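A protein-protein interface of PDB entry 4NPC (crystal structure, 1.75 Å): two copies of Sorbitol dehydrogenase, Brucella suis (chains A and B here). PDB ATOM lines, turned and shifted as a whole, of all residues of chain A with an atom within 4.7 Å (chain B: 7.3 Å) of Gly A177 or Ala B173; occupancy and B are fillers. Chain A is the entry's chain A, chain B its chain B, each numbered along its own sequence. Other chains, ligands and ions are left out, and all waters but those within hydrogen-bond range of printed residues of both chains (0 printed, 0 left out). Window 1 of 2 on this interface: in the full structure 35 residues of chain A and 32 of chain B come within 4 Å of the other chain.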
ATOM      1  N   LEU A 130      31.786  12.456 -32.623  1.00  0.00           N
ATOM      2  CA  LEU A 130      31.929  12.199 -31.193  1.00  0.00           C
ATOM      3  C   LEU A 130      33.204  12.819 -30.644  1.00  0.00           C
ATOM      4  O   LEU A 130      33.134  13.711 -29.780  1.00  0.00           O
ATOM      5  CB  LEU A 130      31.818  10.709 -30.873  1.00  0.00           C
ATOM      6  CG  LEU A 130      31.840  10.310 -29.396  1.00  0.00           C
ATOM      7  CD1 LEU A 130      30.838  11.055 -28.557  1.00  0.00           C
ATOM      8  CD2 LEU A 130      31.647   8.798 -29.316  1.00  0.00           C
ATOM      9  N   CYS A 172      24.384   6.196 -35.148  1.00  0.00           N
ATOM     10  CA  CYS A 172      23.718   5.987 -33.857  1.00  0.00           C
ATOM     11  C   CYS A 172      24.762   5.863 -32.737  1.00  0.00           C
ATOM     12  O   CYS A 172      24.625   6.421 -31.658  1.00  0.00           O
ATOM     13  CB  CYS A 172      22.812   4.758 -33.890  1.00  0.00           C
ATOM     14  SG  CYS A 172      21.344   4.991 -34.901  1.00  0.00           S
ATOM     15  N   ALA A 173      25.810   5.063 -32.956  1.00  0.00           N
ATOM     16  CA  ALA A 173      26.863   4.996 -31.935  1.00  0.00           C
ATOM     17  C   ALA A 173      27.373   6.380 -31.569  1.00  0.00           C
ATOM     18  O   ALA A 173      27.521   6.733 -30.377  1.00  0.00           O
ATOM     19  CB  ALA A 173      28.014   4.156 -32.431  1.00  0.00           C
ATOM     20  N   SER A 174      27.656   7.176 -32.592  1.00  0.00           N
ATOM     21  CA  SER A 174      28.206   8.536 -32.390  1.00  0.00           C
ATOM     22  C   SER A 174      27.221   9.439 -31.637  1.00  0.00           C
ATOM     23  O   SER A 174      27.623  10.165 -30.732  1.00  0.00           O
ATOM     24  CB  SER A 174      28.710   9.201 -33.699  1.00  0.00           C
ATOM     25  OG  SER A 174      27.657   9.706 -34.494  1.00  0.00           O
ATOM     26  N   LYS A 175      25.934   9.352 -31.966  1.00  0.00           N
ATOM     27  CA  LYS A 175      24.949  10.278 -31.396  1.00  0.00           C
ATOM     28  C   LYS A 175      24.487   9.890 -29.994  1.00  0.00           C
ATOM     29  O   LYS A 175      24.315  10.756 -29.149  1.00  0.00           O
ATOM     30  CB  LYS A 175      23.783  10.428 -32.380  1.00  0.00           C
ATOM     31  CG  LYS A 175      24.195  11.113 -33.698  1.00  0.00           C
ATOM     32  CD  LYS A 175      24.804  12.487 -33.478  1.00  0.00           C
ATOM     33  CE  LYS A 175      24.875  13.289 -34.776  1.00  0.00           C
ATOM     34  NZ  LYS A 175      25.369  14.695 -34.577  1.00  0.00           N
ATOM     35  N   PHE A 176      24.326   8.591 -29.721  1.00  0.00           N
ATOM     36  CA  PHE A 176      24.140   8.124 -28.369  1.00  0.00           C
ATOM     37  C   PHE A 176      25.357   8.582 -27.531  1.00  0.00           C
ATOM     38  O   PHE A 176      25.226   9.079 -26.408  1.00  0.00           O
ATOM     39  CB  PHE A 176      24.049   6.576 -28.263  1.00  0.00           C
ATOM     40  CG  PHE A 176      22.655   5.983 -28.489  1.00  0.00           C
ATOM     41  CD1 PHE A 176      22.020   6.016 -29.704  1.00  0.00           C
ATOM     42  CD2 PHE A 176      22.005   5.307 -27.467  1.00  0.00           C
ATOM     43  CE1 PHE A 176      20.785   5.418 -29.911  1.00  0.00           C
ATOM     44  CE2 PHE A 176      20.757   4.738 -27.642  1.00  0.00           C
ATOM     45  CZ  PHE A 176      20.141   4.776 -28.858  1.00  0.00           C
ATOM     46  N   GLY A 177      26.549   8.392 -28.088  1.00  0.00           N
ATOM     47  CA  GLY A 177      27.783   8.822 -27.389  1.00  0.00           C
ATOM     48  C   GLY A 177      27.800  10.290 -27.087  1.00  0.00           C
ATOM     49  O   GLY A 177      28.240  10.672 -26.005  1.00  0.00           O
ATOM     50  N   VAL A 178      27.372  11.107 -28.035  1.00  0.00           N
ATOM     51  CA  VAL A 178      27.368  12.556 -27.838  1.00  0.00           C
ATOM     52  C   VAL A 178      26.477  12.923 -26.618  1.00  0.00           C
ATOM     53  O   VAL A 178      26.808  13.813 -25.830  1.00  0.00           O
ATOM     54  CB  VAL A 178      26.924  13.347 -29.099  1.00  0.00           C
ATOM     55  CG1 VAL A 178      26.554  14.791 -28.764  1.00  0.00           C
ATOM     56  CG2 VAL A 178      28.030  13.306 -30.150  1.00  0.00           C
ATOM     57  N   ILE A 179      25.359  12.270 -26.501  1.00  0.00           N
ATOM     58  CA  ILE A 179      24.441  12.538 -25.421  1.00  0.00           C
ATOM     59  C   ILE A 179      25.103  12.132 -24.070  1.00  0.00           C
ATOM     60  O   ILE A 179      25.072  12.931 -23.097  1.00  0.00           O
ATOM     61  CB  ILE A 179      23.067  11.847 -25.665  1.00  0.00           C
ATOM     62  CG1 ILE A 179      22.374  12.462 -26.862  1.00  0.00           C
ATOM     63  CG2 ILE A 179      22.207  11.867 -24.405  1.00  0.00           C
ATOM     64  CD1 ILE A 179      21.142  11.691 -27.349  1.00  0.00           C
ATOM     65  N   GLY A 180      25.664  10.930 -23.967  1.00  0.00           N
ATOM     66  CA  GLY A 180      26.318  10.541 -22.698  1.00  0.00           C
ATOM     67  C   GLY A 180      27.460  11.467 -22.336  1.00  0.00           C
ATOM     68  O   GLY A 180      27.657  11.815 -21.161  1.00  0.00           O
ATOM     69  N   MET A 181      28.276  11.786 -23.341  1.00  0.00           N
ATOM     70  CA  MET A 181      29.355  12.715 -23.160  1.00  0.00           C
ATOM     71  C   MET A 181      28.856  14.079 -22.628  1.00  0.00           C
ATOM     72  O   MET A 181      29.404  14.615 -21.659  1.00  0.00           O
ATOM     73  CB  MET A 181      30.073  12.928 -24.517  1.00  0.00           C
ATOM     74  CG  MET A 181      31.303  13.799 -24.440  1.00  0.00           C
ATOM     75  SD  MET A 181      31.658  14.571 -26.035  1.00  0.00           S
ATOM     76  CE  MET A 181      30.437  15.840 -26.048  1.00  0.00           C
ATOM     77  N   TRP B 122      40.923   9.560 -23.726  1.00  0.00           N
ATOM     78  CA  TRP B 122      39.764   9.518 -24.631  1.00  0.00           C
ATOM     79  C   TRP B 122      39.953   8.432 -25.696  1.00  0.00           C
ATOM     80  O   TRP B 122      39.086   7.542 -25.869  1.00  0.00           O
ATOM     81  CB  TRP B 122      39.529  10.883 -25.258  1.00  0.00           C
ATOM     82  CG  TRP B 122      38.483  10.827 -26.332  1.00  0.00           C
ATOM     83  CD1 TRP B 122      38.661  10.475 -27.634  1.00  0.00           C
ATOM     84  CD2 TRP B 122      37.085  11.053 -26.146  1.00  0.00           C
ATOM     85  NE1 TRP B 122      37.441  10.486 -28.295  1.00  0.00           N
ATOM     86  CE2 TRP B 122      36.462  10.825 -27.391  1.00  0.00           C
ATOM     87  CE3 TRP B 122      36.298  11.413 -25.039  1.00  0.00           C
ATOM     88  CZ2 TRP B 122      35.101  10.965 -27.559  1.00  0.00           C
ATOM     89  CZ3 TRP B 122      34.932  11.532 -25.212  1.00  0.00           C
ATOM     90  CH2 TRP B 122      34.355  11.339 -26.468  1.00  0.00           C
ATOM     91  N   THR B 125      39.992   4.719 -24.542  1.00  0.00           N
ATOM     92  CA  THR B 125      38.670   4.320 -24.117  1.00  0.00           C
ATOM     93  C   THR B 125      37.761   4.026 -25.322  1.00  0.00           C
ATOM     94  O   THR B 125      37.107   2.970 -25.407  1.00  0.00           O
ATOM     95  CB  THR B 125      38.009   5.400 -23.232  1.00  0.00           C
ATOM     96  OG1 THR B 125      38.838   5.683 -22.069  1.00  0.00           O
ATOM     97  CG2 THR B 125      36.617   4.976 -22.749  1.00  0.00           C
ATOM     98  N   ILE B 126      37.659   4.992 -26.234  1.00  0.00           N
ATOM     99  CA  ILE B 126      36.805   4.793 -27.406  1.00  0.00           C
ATOM    100  C   ILE B 126      37.265   3.602 -28.245  1.00  0.00           C
ATOM    101  O   ILE B 126      36.438   2.789 -28.713  1.00  0.00           O
ATOM    102  CB  ILE B 126      36.726   6.067 -28.231  1.00  0.00           C
ATOM    103  CG1 ILE B 126      36.118   7.219 -27.425  1.00  0.00           C
ATOM    104  CG2 ILE B 126      35.995   5.843 -29.545  1.00  0.00           C
ATOM    105  CD1 ILE B 126      34.686   7.010 -26.948  1.00  0.00           C
ATOM    106  N   LEU B 130      34.389   1.021 -27.523  1.00  0.00           N
ATOM    107  CA  LEU B 130      33.381   1.266 -28.548  1.00  0.00           C
ATOM    108  C   LEU B 130      33.800   0.678 -29.884  1.00  0.00           C
ATOM    109  O   LEU B 130      33.109  -0.200 -30.440  1.00  0.00           O
ATOM    110  CB  LEU B 130      33.097   2.782 -28.666  1.00  0.00           C
ATOM    111  CG  LEU B 130      31.976   3.192 -29.638  1.00  0.00           C
ATOM    112  CD1 LEU B 130      30.691   2.423 -29.404  1.00  0.00           C
ATOM    113  CD2 LEU B 130      31.747   4.702 -29.558  1.00  0.00           C
ATOM    114  N   ALA B 160      27.015   3.391 -16.461  1.00  0.00           N
ATOM    115  CA  ALA B 160      27.498   4.611 -17.106  1.00  0.00           C
ATOM    116  C   ALA B 160      27.029   4.776 -18.581  1.00  0.00           C
ATOM    117  O   ALA B 160      27.376   5.780 -19.211  1.00  0.00           O
ATOM    118  CB  ALA B 160      28.986   4.668 -17.012  1.00  0.00           C
ATOM    119  N   GLY B 161      26.315   3.792 -19.116  1.00  0.00           N
ATOM    120  CA  GLY B 161      25.606   3.895 -20.388  1.00  0.00           C
ATOM    121  C   GLY B 161      24.216   4.520 -20.236  1.00  0.00           C
ATOM    122  O   GLY B 161      23.524   4.755 -21.242  1.00  0.00           O
ATOM    123  N   HIS B 168      34.019  10.469 -15.662  1.00  0.00           N
ATOM    124  CA  HIS B 168      33.772   9.419 -16.638  1.00  0.00           C
ATOM    125  C   HIS B 168      33.360   9.986 -17.993  1.00  0.00           C
ATOM    126  O   HIS B 168      32.618   9.333 -18.745  1.00  0.00           O
ATOM    127  CB  HIS B 168      32.658   8.482 -16.156  1.00  0.00           C
ATOM    128  CG  HIS B 168      33.047   7.613 -14.994  1.00  0.00           C
ATOM    129  ND1 HIS B 168      33.396   8.124 -13.762  1.00  0.00           N
ATOM    130  CD2 HIS B 168      33.093   6.265 -14.864  1.00  0.00           C
ATOM    131  CE1 HIS B 168      33.643   7.134 -12.934  1.00  0.00           C
ATOM    132  NE2 HIS B 168      33.488   5.999 -13.578  1.00  0.00           N
ATOM    133  N   VAL B 169      33.825  11.168 -18.369  1.00  0.00           N
ATOM    134  CA  VAL B 169      33.334  11.666 -19.680  1.00  0.00           C
ATOM    135  C   VAL B 169      33.656  10.739 -20.855  1.00  0.00           C
ATOM    136  O   VAL B 169      32.779  10.522 -21.735  1.00  0.00           O
ATOM    137  CB  VAL B 169      33.791  13.136 -19.954  1.00  0.00           C
ATOM    138  CG1 VAL B 169      35.283  13.233 -20.201  1.00  0.00           C
ATOM    139  CG2 VAL B 169      33.016  13.728 -21.123  1.00  0.00           C
ATOM    140  N   ALA B 170      34.859  10.185 -20.911  1.00  0.00           N
ATOM    141  CA  ALA B 170      35.190   9.253 -22.009  1.00  0.00           C
ATOM    142  C   ALA B 170      34.471   7.914 -21.835  1.00  0.00           C
ATOM    143  O   ALA B 170      33.953   7.326 -22.797  1.00  0.00           O
ATOM    144  CB  ALA B 170      36.694   9.040 -22.086  1.00  0.00           C
ATOM    145  N   TYR B 171      34.417   7.448 -20.589  1.00  0.00           N
ATOM    146  CA  TYR B 171      33.782   6.156 -20.289  1.00  0.00           C
ATOM    147  C   TYR B 171      32.308   6.162 -20.635  1.00  0.00           C
ATOM    148  O   TYR B 171      31.803   5.254 -21.356  1.00  0.00           O
ATOM    149  CB  TYR B 171      34.031   5.800 -18.816  1.00  0.00           C
ATOM    150  CG  TYR B 171      33.670   4.384 -18.474  1.00  0.00           C
ATOM    151  CD1 TYR B 171      34.511   3.327 -18.815  1.00  0.00           C
ATOM    152  CD2 TYR B 171      32.462   4.090 -17.826  1.00  0.00           C
ATOM    153  CE1 TYR B 171      34.159   2.002 -18.505  1.00  0.00           C
ATOM    154  CE2 TYR B 171      32.118   2.793 -17.506  1.00  0.00           C
ATOM    155  CZ  TYR B 171      32.978   1.757 -17.831  1.00  0.00           C
ATOM    156  OH  TYR B 171      32.649   0.442 -17.494  1.00  0.00           O
ATOM    157  N   CYS B 172      31.596   7.198 -20.164  1.00  0.00           N
ATOM    158  CA  CYS B 172      30.159   7.374 -20.484  1.00  0.00           C
ATOM    159  C   CYS B 172      29.932   7.540 -21.971  1.00  0.00           C
ATOM    160  O   CYS B 172      29.007   6.957 -22.559  1.00  0.00           O
ATOM    161  CB  CYS B 172      29.600   8.612 -19.727  1.00  0.00           C
ATOM    162  SG  CYS B 172      29.459   8.353 -17.934  1.00  0.00           S
ATOM    163  N   ALA B 173      30.760   8.344 -22.635  1.00  0.00           N
ATOM    164  CA  ALA B 173      30.612   8.460 -24.088  1.00  0.00           C
ATOM    165  C   ALA B 173      30.716   7.046 -24.757  1.00  0.00           C
ATOM    166  O   ALA B 173      29.915   6.690 -25.629  1.00  0.00           O
ATOM    167  CB  ALA B 173      31.676   9.345 -24.657  1.00  0.00           C
ATOM    168  N   SER B 174      31.699   6.257 -24.343  1.00  0.00           N
ATOM    169  CA  SER B 174      31.904   4.909 -24.911  1.00  0.00           C
ATOM    170  C   SER B 174      30.759   3.955 -24.597  1.00  0.00           C
ATOM    171  O   SER B 174      30.367   3.184 -25.471  1.00  0.00           O
ATOM    172  CB  SER B 174      33.251   4.291 -24.462  1.00  0.00           C
ATOM    173  OG  SER B 174      33.231   3.775 -23.150  1.00  0.00           O
ATOM    174  N   LYS B 175      30.162   4.081 -23.405  1.00  0.00           N
ATOM    175  CA  LYS B 175      29.151   3.128 -22.957  1.00  0.00           C
ATOM    176  C   LYS B 175      27.771   3.483 -23.485  1.00  0.00           C
ATOM    177  O   LYS B 175      27.035   2.577 -23.939  1.00  0.00           O
ATOM    178  CB  LYS B 175      29.149   2.930 -21.452  1.00  0.00           C
ATOM    179  CG  LYS B 175      30.422   2.230 -20.914  1.00  0.00           C
ATOM    180  CD  LYS B 175      30.722   0.902 -21.597  1.00  0.00           C
ATOM    181  CE  LYS B 175      31.817   0.107 -20.884  1.00  0.00           C
ATOM    182  NZ  LYS B 175      31.884  -1.294 -21.373  1.00  0.00           N
ATOM    183  N   PHE B 176      27.393   4.771 -23.460  1.00  0.00           N
ATOM    184  CA  PHE B 176      26.228   5.195 -24.247  1.00  0.00           C
ATOM    185  C   PHE B 176      26.351   4.753 -25.724  1.00  0.00           C
ATOM    186  O   PHE B 176      25.397   4.246 -26.334  1.00  0.00           O
ATOM    187  CB  PHE B 176      26.052   6.742 -24.180  1.00  0.00           C
ATOM    188  CG  PHE B 176      25.326   7.255 -22.944  1.00  0.00           C
ATOM    189  CD1 PHE B 176      25.906   7.244 -21.673  1.00  0.00           C
ATOM    190  CD2 PHE B 176      24.098   7.889 -23.075  1.00  0.00           C
ATOM    191  CE1 PHE B 176      25.247   7.783 -20.551  1.00  0.00           C
ATOM    192  CE2 PHE B 176      23.422   8.385 -21.960  1.00  0.00           C
ATOM    193  CZ  PHE B 176      24.010   8.378 -20.705  1.00  0.00           C
ATOM    194  N   GLY B 177      27.522   4.978 -26.325  1.00  0.00           N
ATOM    195  CA  GLY B 177      27.800   4.571 -27.694  1.00  0.00           C
ATOM    196  C   GLY B 177      27.608   3.094 -27.933  1.00  0.00           C
ATOM    197  O   GLY B 177      26.998   2.717 -28.950  1.00  0.00           O
ATOM    198  N   VAL B 178      28.140   2.261 -27.034  1.00  0.00           N
ATOM    199  CA  VAL B 178      27.969   0.798 -27.130  1.00  0.00           C
ATOM    200  C   VAL B 178      26.485   0.394 -27.193  1.00  0.00           C
ATOM    201  O   VAL B 178      26.118  -0.511 -27.994  1.00  0.00           O
ATOM    202  CB  VAL B 178      28.662   0.058 -25.968  1.00  0.00           C
ATOM    203  CG1 VAL B 178      28.160  -1.365 -25.791  1.00  0.00           C
ATOM    204  CG2 VAL B 178      30.158   0.070 -26.245  1.00  0.00           C
ATOM    205  N   ILE B 179      25.638   1.066 -26.393  1.00  0.00           N
ATOM    206  CA  ILE B 179      24.197   0.761 -26.363  1.00  0.00           C
ATOM    207  C   ILE B 179      23.536   1.126 -27.690  1.00  0.00           C
ATOM    208  O   ILE B 179      22.823   0.309 -28.282  1.00  0.00           O
ATOM    209  CB  ILE B 179      23.525   1.433 -25.156  1.00  0.00           C
ATOM    210  CG1 ILE B 179      24.092   0.814 -23.888  1.00  0.00           C
ATOM    211  CG2 ILE B 179      22.034   1.306 -25.275  1.00  0.00           C
ATOM    212  CD1 ILE B 179      23.717   1.490 -22.598  1.00  0.00           C
ATOM    213  N   GLY B 180      23.806   2.345 -28.181  1.00  0.00           N
ATOM    214  CA  GLY B 180      23.280   2.784 -29.486  1.00  0.00           C
ATOM    215  C   GLY B 180      23.722   1.899 -30.638  1.00  0.00           C
ATOM    216  O   GLY B 180      22.929   1.533 -31.481  1.00  0.00           O
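CG of Leu A130 touches CZ2 of Trp B122, at 3.8 Å.
Ala A173 touches Gly B177 (O to CA, 3.5 Å).
CB of Phe A176 touches O of Phe B176, 3.3 Å away.
Phe A176 touches Gly B180 (CG to CA, 3.4 Å).
Gly A177 touches Ala B173 (CA to O, 3.5 Å).
N of Gly B177 touches N of Gly A177, 3.96 Å away.
Gly A180 touches Phe B176 (CA to CG, 3.4 Å).
CG2 of Val B169 touches CG of Met A181, at 3.7 Å.
Met A181 touches Ala B173.
Hydrophobic or aromatic side chains of chain A within 4 Å of the printed part of chain B: Leu A130, Ala A173, Phe A176 and Met A181.
Hydrophobic or aromatic side chains of chain B that line the printed part of chain A: Trp B122, Val B169, Ala B173 and Phe B176.
Along chain B the printed residues that touch a printed residue of chain A span positions 122 to 180.
Among the printed residues, 9 pairs touch across the chains.
Printed residues of chain B within 4 Å of Leu A130: Trp B122.
Printed residues of chain B within 4 Å of Gly A180: Phe B176.
Printed residues of chain A within 4 Å of Val B169: Met A181.
Ala B173 touches just these residues of chain A: Gly A177 (3.5 Å) and Met A181 (3.9 Å).
The nearest residue of chain A that does not touch Ala B173 is Leu A130 (4.3 Å).
The nearest printed residue of chain A that does not touch Gly B177 is Phe A176 (4.3 Å).
Ala A173 touches Gly B177, and with the chains exchanged Gly A177 touches Ala B173.
Phe B176 touches its own counterpart, Phe A176.
Phe A176 touches Gly B180, and with the chains exchanged Gly A180 touches Phe B176.
Gly B177 touches its own counterpart, Gly A177.
Of the 9 pairs that touch across the chains among the printed residues, 6 have their exchanged pair printed and touching as well.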
